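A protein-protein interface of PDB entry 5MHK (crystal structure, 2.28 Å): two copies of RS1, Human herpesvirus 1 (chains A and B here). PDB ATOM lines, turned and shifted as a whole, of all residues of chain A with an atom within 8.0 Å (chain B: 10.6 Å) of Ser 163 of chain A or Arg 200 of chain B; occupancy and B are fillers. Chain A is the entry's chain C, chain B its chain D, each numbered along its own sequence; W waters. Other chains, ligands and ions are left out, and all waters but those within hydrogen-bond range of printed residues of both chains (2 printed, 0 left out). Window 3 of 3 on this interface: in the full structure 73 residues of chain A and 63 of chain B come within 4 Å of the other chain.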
ATOM      1  N   ASN A 160     -24.195  14.292 -21.055  1.00  0.00           N
ATOM      2  CA  ASN A 160     -22.899  13.643 -21.185  1.00  0.00           C
ATOM      3  C   ASN A 160     -23.064  12.133 -21.064  1.00  0.00           C
ATOM      4  O   ASN A 160     -23.653  11.634 -20.100  1.00  0.00           O
ATOM      5  CB  ASN A 160     -21.933  14.168 -20.124  1.00  0.00           C
ATOM      6  CG  ASN A 160     -20.485  13.863 -20.452  1.00  0.00           C
ATOM      7  OD1 ASN A 160     -20.192  13.058 -21.335  1.00  0.00           O
ATOM      8  ND2 ASN A 160     -19.570  14.517 -19.746  1.00  0.00           N
ATOM      9  N   SER A 161     -22.536  11.407 -22.045  1.00  0.00           N
ATOM     10  CA  SER A 161     -22.667   9.960 -22.113  1.00  0.00           C
ATOM     11  C   SER A 161     -21.311   9.340 -22.407  1.00  0.00           C
ATOM     12  O   SER A 161     -20.547   9.852 -23.230  1.00  0.00           O
ATOM     13  CB  SER A 161     -23.677   9.542 -23.190  1.00  0.00           C
ATOM     14  OG  SER A 161     -23.694   8.135 -23.358  1.00  0.00           O
ATOM     15  N   SER A 162     -21.024   8.229 -21.726  1.00  0.00           N
ATOM     16  CA  SER A 162     -19.725   7.575 -21.818  1.00  0.00           C
ATOM     17  C   SER A 162     -19.450   6.976 -23.189  1.00  0.00           C
ATOM     18  O   SER A 162     -18.294   6.651 -23.480  1.00  0.00           O
ATOM     19  CB  SER A 162     -19.623   6.483 -20.752  1.00  0.00           C
ATOM     20  OG  SER A 162     -19.870   7.013 -19.459  1.00  0.00           O
ATOM     21  N   SER A 163     -20.468   6.825 -24.034  1.00  0.00           N
ATOM     22  CA  SER A 163     -20.315   6.141 -25.309  1.00  0.00           C
ATOM     23  C   SER A 163     -19.966   7.070 -26.465  1.00  0.00           C
ATOM     24  O   SER A 163     -19.581   6.581 -27.532  1.00  0.00           O
ATOM     25  CB  SER A 163     -21.597   5.377 -25.652  1.00  0.00           C
ATOM     26  OG  SER A 163     -22.700   6.260 -25.757  1.00  0.00           O
ATOM     27  N   PHE A 164     -20.088   8.384 -26.291  1.00  0.00           N
ATOM     28  CA  PHE A 164     -19.856   9.294 -27.405  1.00  0.00           C
ATOM     29  C   PHE A 164     -18.370   9.430 -27.702  1.00  0.00           C
ATOM     30  O   PHE A 164     -17.539   9.491 -26.791  1.00  0.00           O
ATOM     31  CB  PHE A 164     -20.418  10.683 -27.095  1.00  0.00           C
ATOM     32  CG  PHE A 164     -21.913  10.737 -26.980  1.00  0.00           C
ATOM     33  CD1 PHE A 164     -22.710   9.756 -27.545  1.00  0.00           C
ATOM     34  CD2 PHE A 164     -22.523  11.787 -26.311  1.00  0.00           C
ATOM     35  CE1 PHE A 164     -24.087   9.817 -27.436  1.00  0.00           C
ATOM     36  CE2 PHE A 164     -23.898  11.853 -26.200  1.00  0.00           C
ATOM     37  CZ  PHE A 164     -24.681  10.869 -26.763  1.00  0.00           C
ATOM     38  N   ILE A 165     -18.035   9.483 -28.987  1.00  0.00           N
ATOM     39  CA  ILE A 165     -16.665   9.765 -29.398  1.00  0.00           C
ATOM     40  C   ILE A 165     -16.494  11.278 -29.376  1.00  0.00           C
ATOM     41  O   ILE A 165     -17.190  12.000 -30.097  1.00  0.00           O
ATOM     42  CB  ILE A 165     -16.361   9.181 -30.785  1.00  0.00           C
ATOM     43  CG1 ILE A 165     -16.411   7.651 -30.739  1.00  0.00           C
ATOM     44  CG2 ILE A 165     -15.004   9.656 -31.276  1.00  0.00           C
ATOM     45  CD1 ILE A 165     -16.369   6.994 -32.100  1.00  0.00           C
ATOM     46  N   THR A 166     -15.571  11.764 -28.547  1.00  0.00           N
ATOM     47  CA  THR A 166     -15.361  13.197 -28.401  1.00  0.00           C
ATOM     48  C   THR A 166     -14.063  13.699 -29.009  1.00  0.00           C
ATOM     49  O   THR A 166     -13.947  14.903 -29.259  1.00  0.00           O
ATOM     50  CB  THR A 166     -15.387  13.595 -26.917  1.00  0.00           C
ATOM     51  OG1 THR A 166     -14.386  12.857 -26.206  1.00  0.00           O
ATOM     52  CG2 THR A 166     -16.754  13.308 -26.310  1.00  0.00           C
ATOM     53  N   GLY A 167     -13.093  12.822 -29.250  1.00  0.00           N
ATOM     54  CA  GLY A 167     -11.782  13.245 -29.685  1.00  0.00           C
ATOM     55  C   GLY A 167     -10.840  13.620 -28.564  1.00  0.00           C
ATOM     56  O   GLY A 167      -9.719  14.068 -28.843  1.00  0.00           O
ATOM     57  N   SER A 168     -11.259  13.464 -27.309  1.00  0.00           N
ATOM     58  CA  SER A 168     -10.397  13.725 -26.163  1.00  0.00           C
ATOM     59  C   SER A 168     -10.963  12.986 -24.961  1.00  0.00           C
ATOM     60  O   SER A 168     -12.135  13.171 -24.617  1.00  0.00           O
ATOM     61  CB  SER A 168     -10.299  15.225 -25.872  1.00  0.00           C
ATOM     62  OG  SER A 168      -9.453  15.473 -24.765  1.00  0.00           O
ATOM     63  N   VAL A 169     -10.135  12.152 -24.328  1.00  0.00           N
ATOM     64  CA  VAL A 169     -10.606  11.364 -23.194  1.00  0.00           C
ATOM     65  C   VAL A 169     -10.678  12.197 -21.920  1.00  0.00           C
ATOM     66  O   VAL A 169     -11.391  11.824 -20.979  1.00  0.00           O
ATOM     67  CB  VAL A 169      -9.706  10.130 -22.992  1.00  0.00           C
ATOM     68  CG1 VAL A 169      -8.330  10.542 -22.488  1.00  0.00           C
ATOM     69  CG2 VAL A 169     -10.362   9.115 -22.059  1.00  0.00           C
ATOM     70  N   MET B 132      -4.551  -2.325 -32.367  1.00  0.00           N
ATOM     71  CA  MET B 132      -5.455  -1.607 -31.472  1.00  0.00           C
ATOM     72  C   MET B 132      -6.829  -2.267 -31.418  1.00  0.00           C
ATOM     73  O   MET B 132      -7.436  -2.361 -30.345  1.00  0.00           O
ATOM     74  CB  MET B 132      -5.573  -0.146 -31.904  1.00  0.00           C
ATOM     75  CG  MET B 132      -4.262   0.623 -31.829  1.00  0.00           C
ATOM     76  SD  MET B 132      -3.594   0.713 -30.154  1.00  0.00           S
ATOM     77  CE  MET B 132      -4.445   2.160 -29.532  1.00  0.00           C
ATOM     78  N   GLN B 136      -8.616  -4.082 -28.073  1.00  0.00           N
ATOM     79  CA  GLN B 136      -9.909  -3.614 -27.585  1.00  0.00           C
ATOM     80  C   GLN B 136     -10.960  -4.716 -27.607  1.00  0.00           C
ATOM     81  O   GLN B 136     -11.794  -4.798 -26.698  1.00  0.00           O
ATOM     82  CB  GLN B 136     -10.396  -2.423 -28.412  1.00  0.00           C
ATOM     83  CG  GLN B 136     -11.780  -1.932 -27.998  1.00  0.00           C
ATOM     84  CD  GLN B 136     -12.178  -0.633 -28.668  1.00  0.00           C
ATOM     85  OE1 GLN B 136     -11.745  -0.335 -29.781  1.00  0.00           O
ATOM     86  NE2 GLN B 136     -13.016   0.147 -27.993  1.00  0.00           N
ATOM     87  N   VAL B 169      -5.002  -2.900 -18.104  1.00  0.00           N
ATOM     88  CA  VAL B 169      -6.257  -2.495 -18.726  1.00  0.00           C
ATOM     89  C   VAL B 169      -6.710  -3.482 -19.798  1.00  0.00           C
ATOM     90  O   VAL B 169      -7.892  -3.488 -20.165  1.00  0.00           O
ATOM     91  CB  VAL B 169      -6.120  -1.068 -19.289  1.00  0.00           C
ATOM     92  CG1 VAL B 169      -5.176  -1.046 -20.477  1.00  0.00           C
ATOM     93  CG2 VAL B 169      -7.481  -0.482 -19.648  1.00  0.00           C
ATOM     94  N   ALA B 193      -0.646   1.951 -24.855  1.00  0.00           N
ATOM     95  CA  ALA B 193      -1.398   1.694 -26.078  1.00  0.00           C
ATOM     96  C   ALA B 193      -2.722   1.002 -25.780  1.00  0.00           C
ATOM     97  O   ALA B 193      -3.734   1.274 -26.437  1.00  0.00           O
ATOM     98  CB  ALA B 193      -0.562   0.856 -27.045  1.00  0.00           C
ATOM     99  N   ALA B 194      -2.735   0.099 -24.796  1.00  0.00           N
ATOM    100  CA  ALA B 194      -3.963  -0.618 -24.470  1.00  0.00           C
ATOM    101  C   ALA B 194      -4.985   0.297 -23.805  1.00  0.00           C
ATOM    102  O   ALA B 194      -6.193   0.148 -24.025  1.00  0.00           O
ATOM    103  CB  ALA B 194      -3.649  -1.820 -23.581  1.00  0.00           C
ATOM    104  N   ALA B 195      -4.524   1.248 -22.988  1.00  0.00           N
ATOM    105  CA  ALA B 195      -5.444   2.202 -22.374  1.00  0.00           C
ATOM    106  C   ALA B 195      -6.114   3.070 -23.429  1.00  0.00           C
ATOM    107  O   ALA B 195      -7.300   3.401 -23.315  1.00  0.00           O
ATOM    108  CB  ALA B 195      -4.706   3.067 -21.353  1.00  0.00           C
ATOM    109  N   VAL B 196      -5.367   3.452 -24.466  1.00  0.00           N
ATOM    110  CA  VAL B 196      -5.951   4.185 -25.584  1.00  0.00           C
ATOM    111  C   VAL B 196      -6.939   3.305 -26.339  1.00  0.00           C
ATOM    112  O   VAL B 196      -8.037   3.747 -26.699  1.00  0.00           O
ATOM    113  CB  VAL B 196      -4.840   4.714 -26.507  1.00  0.00           C
ATOM    114  CG1 VAL B 196      -5.436   5.288 -27.784  1.00  0.00           C
ATOM    115  CG2 VAL B 196      -4.002   5.760 -25.784  1.00  0.00           C
ATOM    116  N   ALA B 197      -6.564   2.046 -26.590  1.00  0.00           N
ATOM    117  CA  ALA B 197      -7.424   1.145 -27.350  1.00  0.00           C
ATOM    118  C   ALA B 197      -8.759   0.914 -26.652  1.00  0.00           C
ATOM    119  O   ALA B 197      -9.800   0.805 -27.312  1.00  0.00           O
ATOM    120  CB  ALA B 197      -6.707  -0.185 -27.585  1.00  0.00           C
ATOM    121  N   MET B 198      -8.754   0.839 -25.321  1.00  0.00           N
ATOM    122  CA  MET B 198      -9.981   0.589 -24.573  1.00  0.00           C
ATOM    123  C   MET B 198     -10.836   1.837 -24.384  1.00  0.00           C
ATOM    124  O   MET B 198     -12.003   1.711 -24.000  1.00  0.00           O
ATOM    125  CB  MET B 198      -9.652  -0.018 -23.205  1.00  0.00           C
ATOM    126  CG  MET B 198      -8.954  -1.372 -23.264  1.00  0.00           C
ATOM    127  SD  MET B 198     -10.001  -2.708 -23.875  1.00  0.00           S
ATOM    128  CE  MET B 198     -11.252  -2.772 -22.597  1.00  0.00           C
ATOM    129  N   SER B 199     -10.295   3.025 -24.642  1.00  0.00           N
ATOM    130  CA  SER B 199     -11.052   4.258 -24.462  1.00  0.00           C
ATOM    131  C   SER B 199     -12.209   4.338 -25.453  1.00  0.00           C
ATOM    132  O   SER B 199     -12.094   3.913 -26.604  1.00  0.00           O
ATOM    133  CB  SER B 199     -10.138   5.472 -24.628  1.00  0.00           C
ATOM    134  OG  SER B 199     -10.871   6.680 -24.524  1.00  0.00           O
ATOM    135  N   ARG B 200     -13.335   4.879 -24.992  1.00  0.00           N
ATOM    136  CA  ARG B 200     -14.513   5.057 -25.830  1.00  0.00           C
ATOM    137  C   ARG B 200     -14.582   6.431 -26.488  1.00  0.00           C
ATOM    138  O   ARG B 200     -15.547   6.705 -27.211  1.00  0.00           O
ATOM    139  CB  ARG B 200     -15.785   4.836 -25.002  1.00  0.00           C
ATOM    140  CG  ARG B 200     -15.809   3.537 -24.212  1.00  0.00           C
ATOM    141  CD  ARG B 200     -17.152   3.324 -23.529  1.00  0.00           C
ATOM    142  NE  ARG B 200     -18.194   2.899 -24.460  1.00  0.00           N
ATOM    143  CZ  ARG B 200     -19.457   2.669 -24.110  1.00  0.00           C
ATOM    144  NH1 ARG B 200     -19.836   2.827 -22.850  1.00  0.00           N
ATOM    145  NH2 ARG B 200     -20.341   2.281 -25.018  1.00  0.00           N
ATOM    146  N   ARG B 201     -13.589   7.296 -26.272  1.00  0.00           N
ATOM    147  CA  ARG B 201     -13.651   8.674 -26.744  1.00  0.00           C
ATOM    148  C   ARG B 201     -12.959   8.909 -28.082  1.00  0.00           C
ATOM    149  O   ARG B 201     -13.052  10.020 -28.613  1.00  0.00           O
ATOM    150  CB  ARG B 201     -13.048   9.622 -25.699  1.00  0.00           C
ATOM    151  CG  ARG B 201     -13.719   9.588 -24.332  1.00  0.00           C
ATOM    152  CD  ARG B 201     -15.224   9.810 -24.433  1.00  0.00           C
ATOM    153  NE  ARG B 201     -15.809  10.163 -23.141  1.00  0.00           N
ATOM    154  CZ  ARG B 201     -17.095  10.444 -22.949  1.00  0.00           C
ATOM    155  NH1 ARG B 201     -17.945  10.411 -23.967  1.00  0.00           N
ATOM    156  NH2 ARG B 201     -17.533  10.761 -21.738  1.00  0.00           N
ATOM    157  N   TYR B 202     -12.271   7.913 -28.636  1.00  0.00           N
ATOM    158  CA  TYR B 202     -11.576   8.058 -29.906  1.00  0.00           C
ATOM    159  C   TYR B 202     -12.104   7.050 -30.919  1.00  0.00           C
ATOM    160  O   TYR B 202     -12.481   5.929 -30.563  1.00  0.00           O
ATOM    161  CB  TYR B 202     -10.066   7.859 -29.726  1.00  0.00           C
ATOM    162  CG  TYR B 202      -9.440   8.785 -28.707  1.00  0.00           C
ATOM    163  CD1 TYR B 202      -9.195  10.120 -29.005  1.00  0.00           C
ATOM    164  CD2 TYR B 202      -9.097   8.322 -27.443  1.00  0.00           C
ATOM    165  CE1 TYR B 202      -8.621  10.966 -28.070  1.00  0.00           C
ATOM    166  CE2 TYR B 202      -8.524   9.159 -26.504  1.00  0.00           C
ATOM    167  CZ  TYR B 202      -8.288  10.479 -26.822  1.00  0.00           C
ATOM    168  OH  TYR B 202      -7.717  11.313 -25.886  1.00  0.00           O
ATOM    169  N   ASP B 203     -12.129   7.453 -32.190  1.00  0.00           N
ATOM    170  CA  ASP B 203     -12.529   6.548 -33.257  1.00  0.00           C
ATOM    171  C   ASP B 203     -11.299   5.812 -33.796  1.00  0.00           C
ATOM    172  O   ASP B 203     -10.190   5.937 -33.269  1.00  0.00           O
ATOM    173  CB  ASP B 203     -13.300   7.296 -34.351  1.00  0.00           C
ATOM    174  CG  ASP B 203     -12.440   8.278 -35.139  1.00  0.00           C
ATOM    175  OD1 ASP B 203     -11.223   8.389 -34.885  1.00  0.00           O
ATOM    176  OD2 ASP B 203     -12.996   8.941 -36.041  1.00  0.00           O
ATOM    177  N   ARG B 204     -11.492   5.043 -34.869  1.00  0.00           N
ATOM    178  CA  ARG B 204     -10.430   4.187 -35.390  1.00  0.00           C
ATOM    179  C   ARG B 204      -9.242   5.003 -35.890  1.00  0.00           C
ATOM    180  O   ARG B 204      -8.085   4.685 -35.590  1.00  0.00           O
ATOM    181  CB  ARG B 204     -10.989   3.313 -36.514  1.00  0.00           C
ATOM    182  CG  ARG B 204      -9.966   2.455 -37.231  1.00  0.00           C
ATOM    183  CD  ARG B 204     -10.636   1.660 -38.344  1.00  0.00           C
ATOM    184  NE  ARG B 204      -9.679   0.908 -39.151  1.00  0.00           N
ATOM    185  CZ  ARG B 204      -9.123  -0.240 -38.778  1.00  0.00           C
ATOM    186  NH1 ARG B 204      -9.429  -0.780 -37.607  1.00  0.00           N
ATOM    187  NH2 ARG B 204      -8.264  -0.850 -39.581  1.00  0.00           N
ATOM    188  N   GLN B 206      -8.370   8.082 -35.095  1.00  0.00           N
ATOM    189  CA  GLN B 206      -7.704   8.782 -34.002  1.00  0.00           C
ATOM    190  C   GLN B 206      -6.796   7.844 -33.216  1.00  0.00           C
ATOM    191  O   GLN B 206      -5.679   8.222 -32.844  1.00  0.00           O
ATOM    192  CB  GLN B 206      -8.743   9.432 -33.088  1.00  0.00           C
ATOM    193  CG  GLN B 206      -9.368  10.689 -33.679  1.00  0.00           C
ATOM    194  CD  GLN B 206     -10.689  11.056 -33.028  1.00  0.00           C
ATOM    195  OE1 GLN B 206     -11.290  10.253 -32.313  1.00  0.00           O
ATOM    196  NE2 GLN B 206     -11.148  12.277 -33.276  1.00  0.00           N
ATOM    197  N   LYS B 207      -7.258   6.621 -32.946  1.00  0.00           N
ATOM    198  CA  LYS B 207      -6.404   5.653 -32.267  1.00  0.00           C
ATOM    199  C   LYS B 207      -5.211   5.263 -33.128  1.00  0.00           C
ATOM    200  O   LYS B 207      -4.134   4.973 -32.596  1.00  0.00           O
ATOM    201  CB  LYS B 207      -7.216   4.420 -31.866  1.00  0.00           C
ATOM    202  CG  LYS B 207      -8.270   4.708 -30.807  1.00  0.00           C
ATOM    203  CD  LYS B 207      -9.081   3.473 -30.444  1.00  0.00           C
ATOM    204  CE  LYS B 207     -10.080   3.791 -29.337  1.00  0.00           C
ATOM    205  NZ  LYS B 207     -10.844   2.592 -28.890  1.00  0.00           N
ATOM    206  N   LEU B 210      -2.608   7.923 -32.566  1.00  0.00           N
ATOM    207  CA  LEU B 210      -1.971   7.774 -31.263  1.00  0.00           C
ATOM    208  C   LEU B 210      -0.999   6.601 -31.238  1.00  0.00           C
ATOM    209  O   LEU B 210       0.026   6.667 -30.552  1.00  0.00           O
ATOM    210  CB  LEU B 210      -3.034   7.621 -30.176  1.00  0.00           C
ATOM    211  CG  LEU B 210      -3.803   8.913 -29.889  1.00  0.00           C
ATOM    212  CD1 LEU B 210      -4.937   8.684 -28.901  1.00  0.00           C
ATOM    213  CD2 LEU B 210      -2.852   9.989 -29.381  1.00  0.00           C
HETATM  214  O   HOH W   1     -17.269   4.966 -28.258  1.00  0.00           O
HETATM  215  O   HOH W   2     -14.200  10.955 -21.040  1.00  0.00           O
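The backbone NH (N) of Thr 166 of chain A is in hydrogen-bond range of the backbone carbonyl oxygen (O) of Arg 201 of chain B (3.1 Å).
The backbone carbonyl oxygen (O) of Phe 164 of chain A lies close to the backbone carbonyl oxygen (O) of Arg 200 of chain B (3.5 Å).
O of Arg 201 of chain B is in hydrogen-bond range of N of Gly 167 of chain A.
The backbone carbonyl oxygen of Phe 164 of chain A sits at hydrogen-bond distance from the guanidinium group of Arg 201 of chain B (3.0 Å).
N of Val 169 of chain A lies within hydrogen-bond range of OH of Tyr 202 of chain B, at 3.0 Å.
O of Ser 161 of chain A lies within hydrogen-bond range of NH1 of Arg 201 of chain B (2.8 Å).
The side-chain hydroxyl of Ser 161 of chain A sits at hydrogen-bond distance from the side-chain hydroxyl of Ser 163 of chain A (3.2 Å).
The side-chain hydroxyl (OG1) of Thr 166 of chain A lies within hydrogen-bond range of the backbone carbonyl oxygen (O) of Ser 168 of chain A.
NZ of Lys 207 of chain B lies within hydrogen-bond range of O of Ser 199 of chain B, 2.9 Å away.
The backbone NH (N) of Gln 206 of chain B lies within hydrogen-bond range of the side-chain carboxylate (OD1) of Asp 203 of chain B, 2.9 Å away.
The backbone NH of Arg 201 of chain B lies within hydrogen-bond range of the side-chain hydroxyl of Ser 199 of chain B (3.3 Å).
Among the printed residues, pairs that only touch across the chains: Asn 160 of chain A with Arg 201 of chain B (3.5 Å), Ser 162 of chain A with Arg 200 of chain B (3.5 Å), Ser 162 of chain A with Arg 201 of chain B (3.8 Å), Ser 163 of chain A with Arg 200 of chain B (3.4 Å), Ile 165 of chain A with Arg 200 of chain B (3.8 Å), Ile 165 of chain A with Arg 201 of chain B (3.3 Å), Ile 165 of chain A with Tyr 202 of chain B (3.9 Å), Ile 165 of chain A with Asp 203 of chain B (3.7 Å), Ile 165 of chain A with Gln 206 of chain B (3.9 Å), Gly 167 of chain A with Tyr 202 of chain B (3.4 Å), Gly 167 of chain A with Gln 206 of chain B (3.8 Å), Ser 168 of chain A with Arg 201 of chain B (3.8 Å), Ser 168 of chain A with Tyr 202 of chain B (3.6 Å), Val 169 of chain A with Ser 199 of chain B (3.5 Å) and Val 169 of chain A with Arg 201 of chain B (3.8 Å).
Of the printed residues of chain B, Asn 160 of chain A touches Arg 201 (3.5 Å).
Printed residues of chain B within 4 Å of Ser 162 of chain A: Arg 200 (3.5 Å) and Arg 201 (3.8 Å).
Ile 165 of chain A touches five residues of chain B.
Of the printed residues of chain B, Thr 166 of chain A touches Arg 201.
Of the printed residues of chain B, Ser 168 of chain A touches Arg 201 (3.8 Å) and Tyr 202 (3.6 Å).
Of chain A, only Val 169 comes within 4 Å of Ser 199 of chain B.
Of the printed residues of chain A, Asp 203 of chain B touches Ile 165.
Of the printed residues of chain A, Gln 206 of chain B touches Ile 165 and Gly 167.
The nearest residue of chain A that does not touch Arg 200 of chain B is Thr 166 of chain A (5.2 Å).
The nearest printed residue of chain A that does not touch Asp 203 of chain B is Gly 167 of chain A (6.2 Å).
Printed residues of chain B that touch a printed residue of chain A: Ser 199, Arg 200, Arg 201, Tyr 202, Asp 203 and Gln 206.
Hydrophobic or aromatic side chains of chain B within 4 Å of the printed part of chain A: Tyr 202.
Hydrophobic or aromatic side chains of chain A within 4 Å of the printed part of chain B: Phe 164, Ile 165 and Val 169.
Among the printed residues, no Asp or Glu carboxylate lies within 4 Å of a Lys or Arg side-chain nitrogen of the other chain.
Position printed for both chains: 169.
Of the 21 pairs that touch across the chains among the printed residues, none has its exchanged pair printed and touching as well.
Water W1 bridges the backbone carbonyl oxygen of Arg 200 of chain B (2.7 Å) and the backbone carbonyl oxygen of Ser 163 of chain A (2.9 Å).
Water W2 lies within hydrogen-bond range of NE of Arg 201 of chain B (2.8 Å) and O of Val 169 of chain A (2.9 Å).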
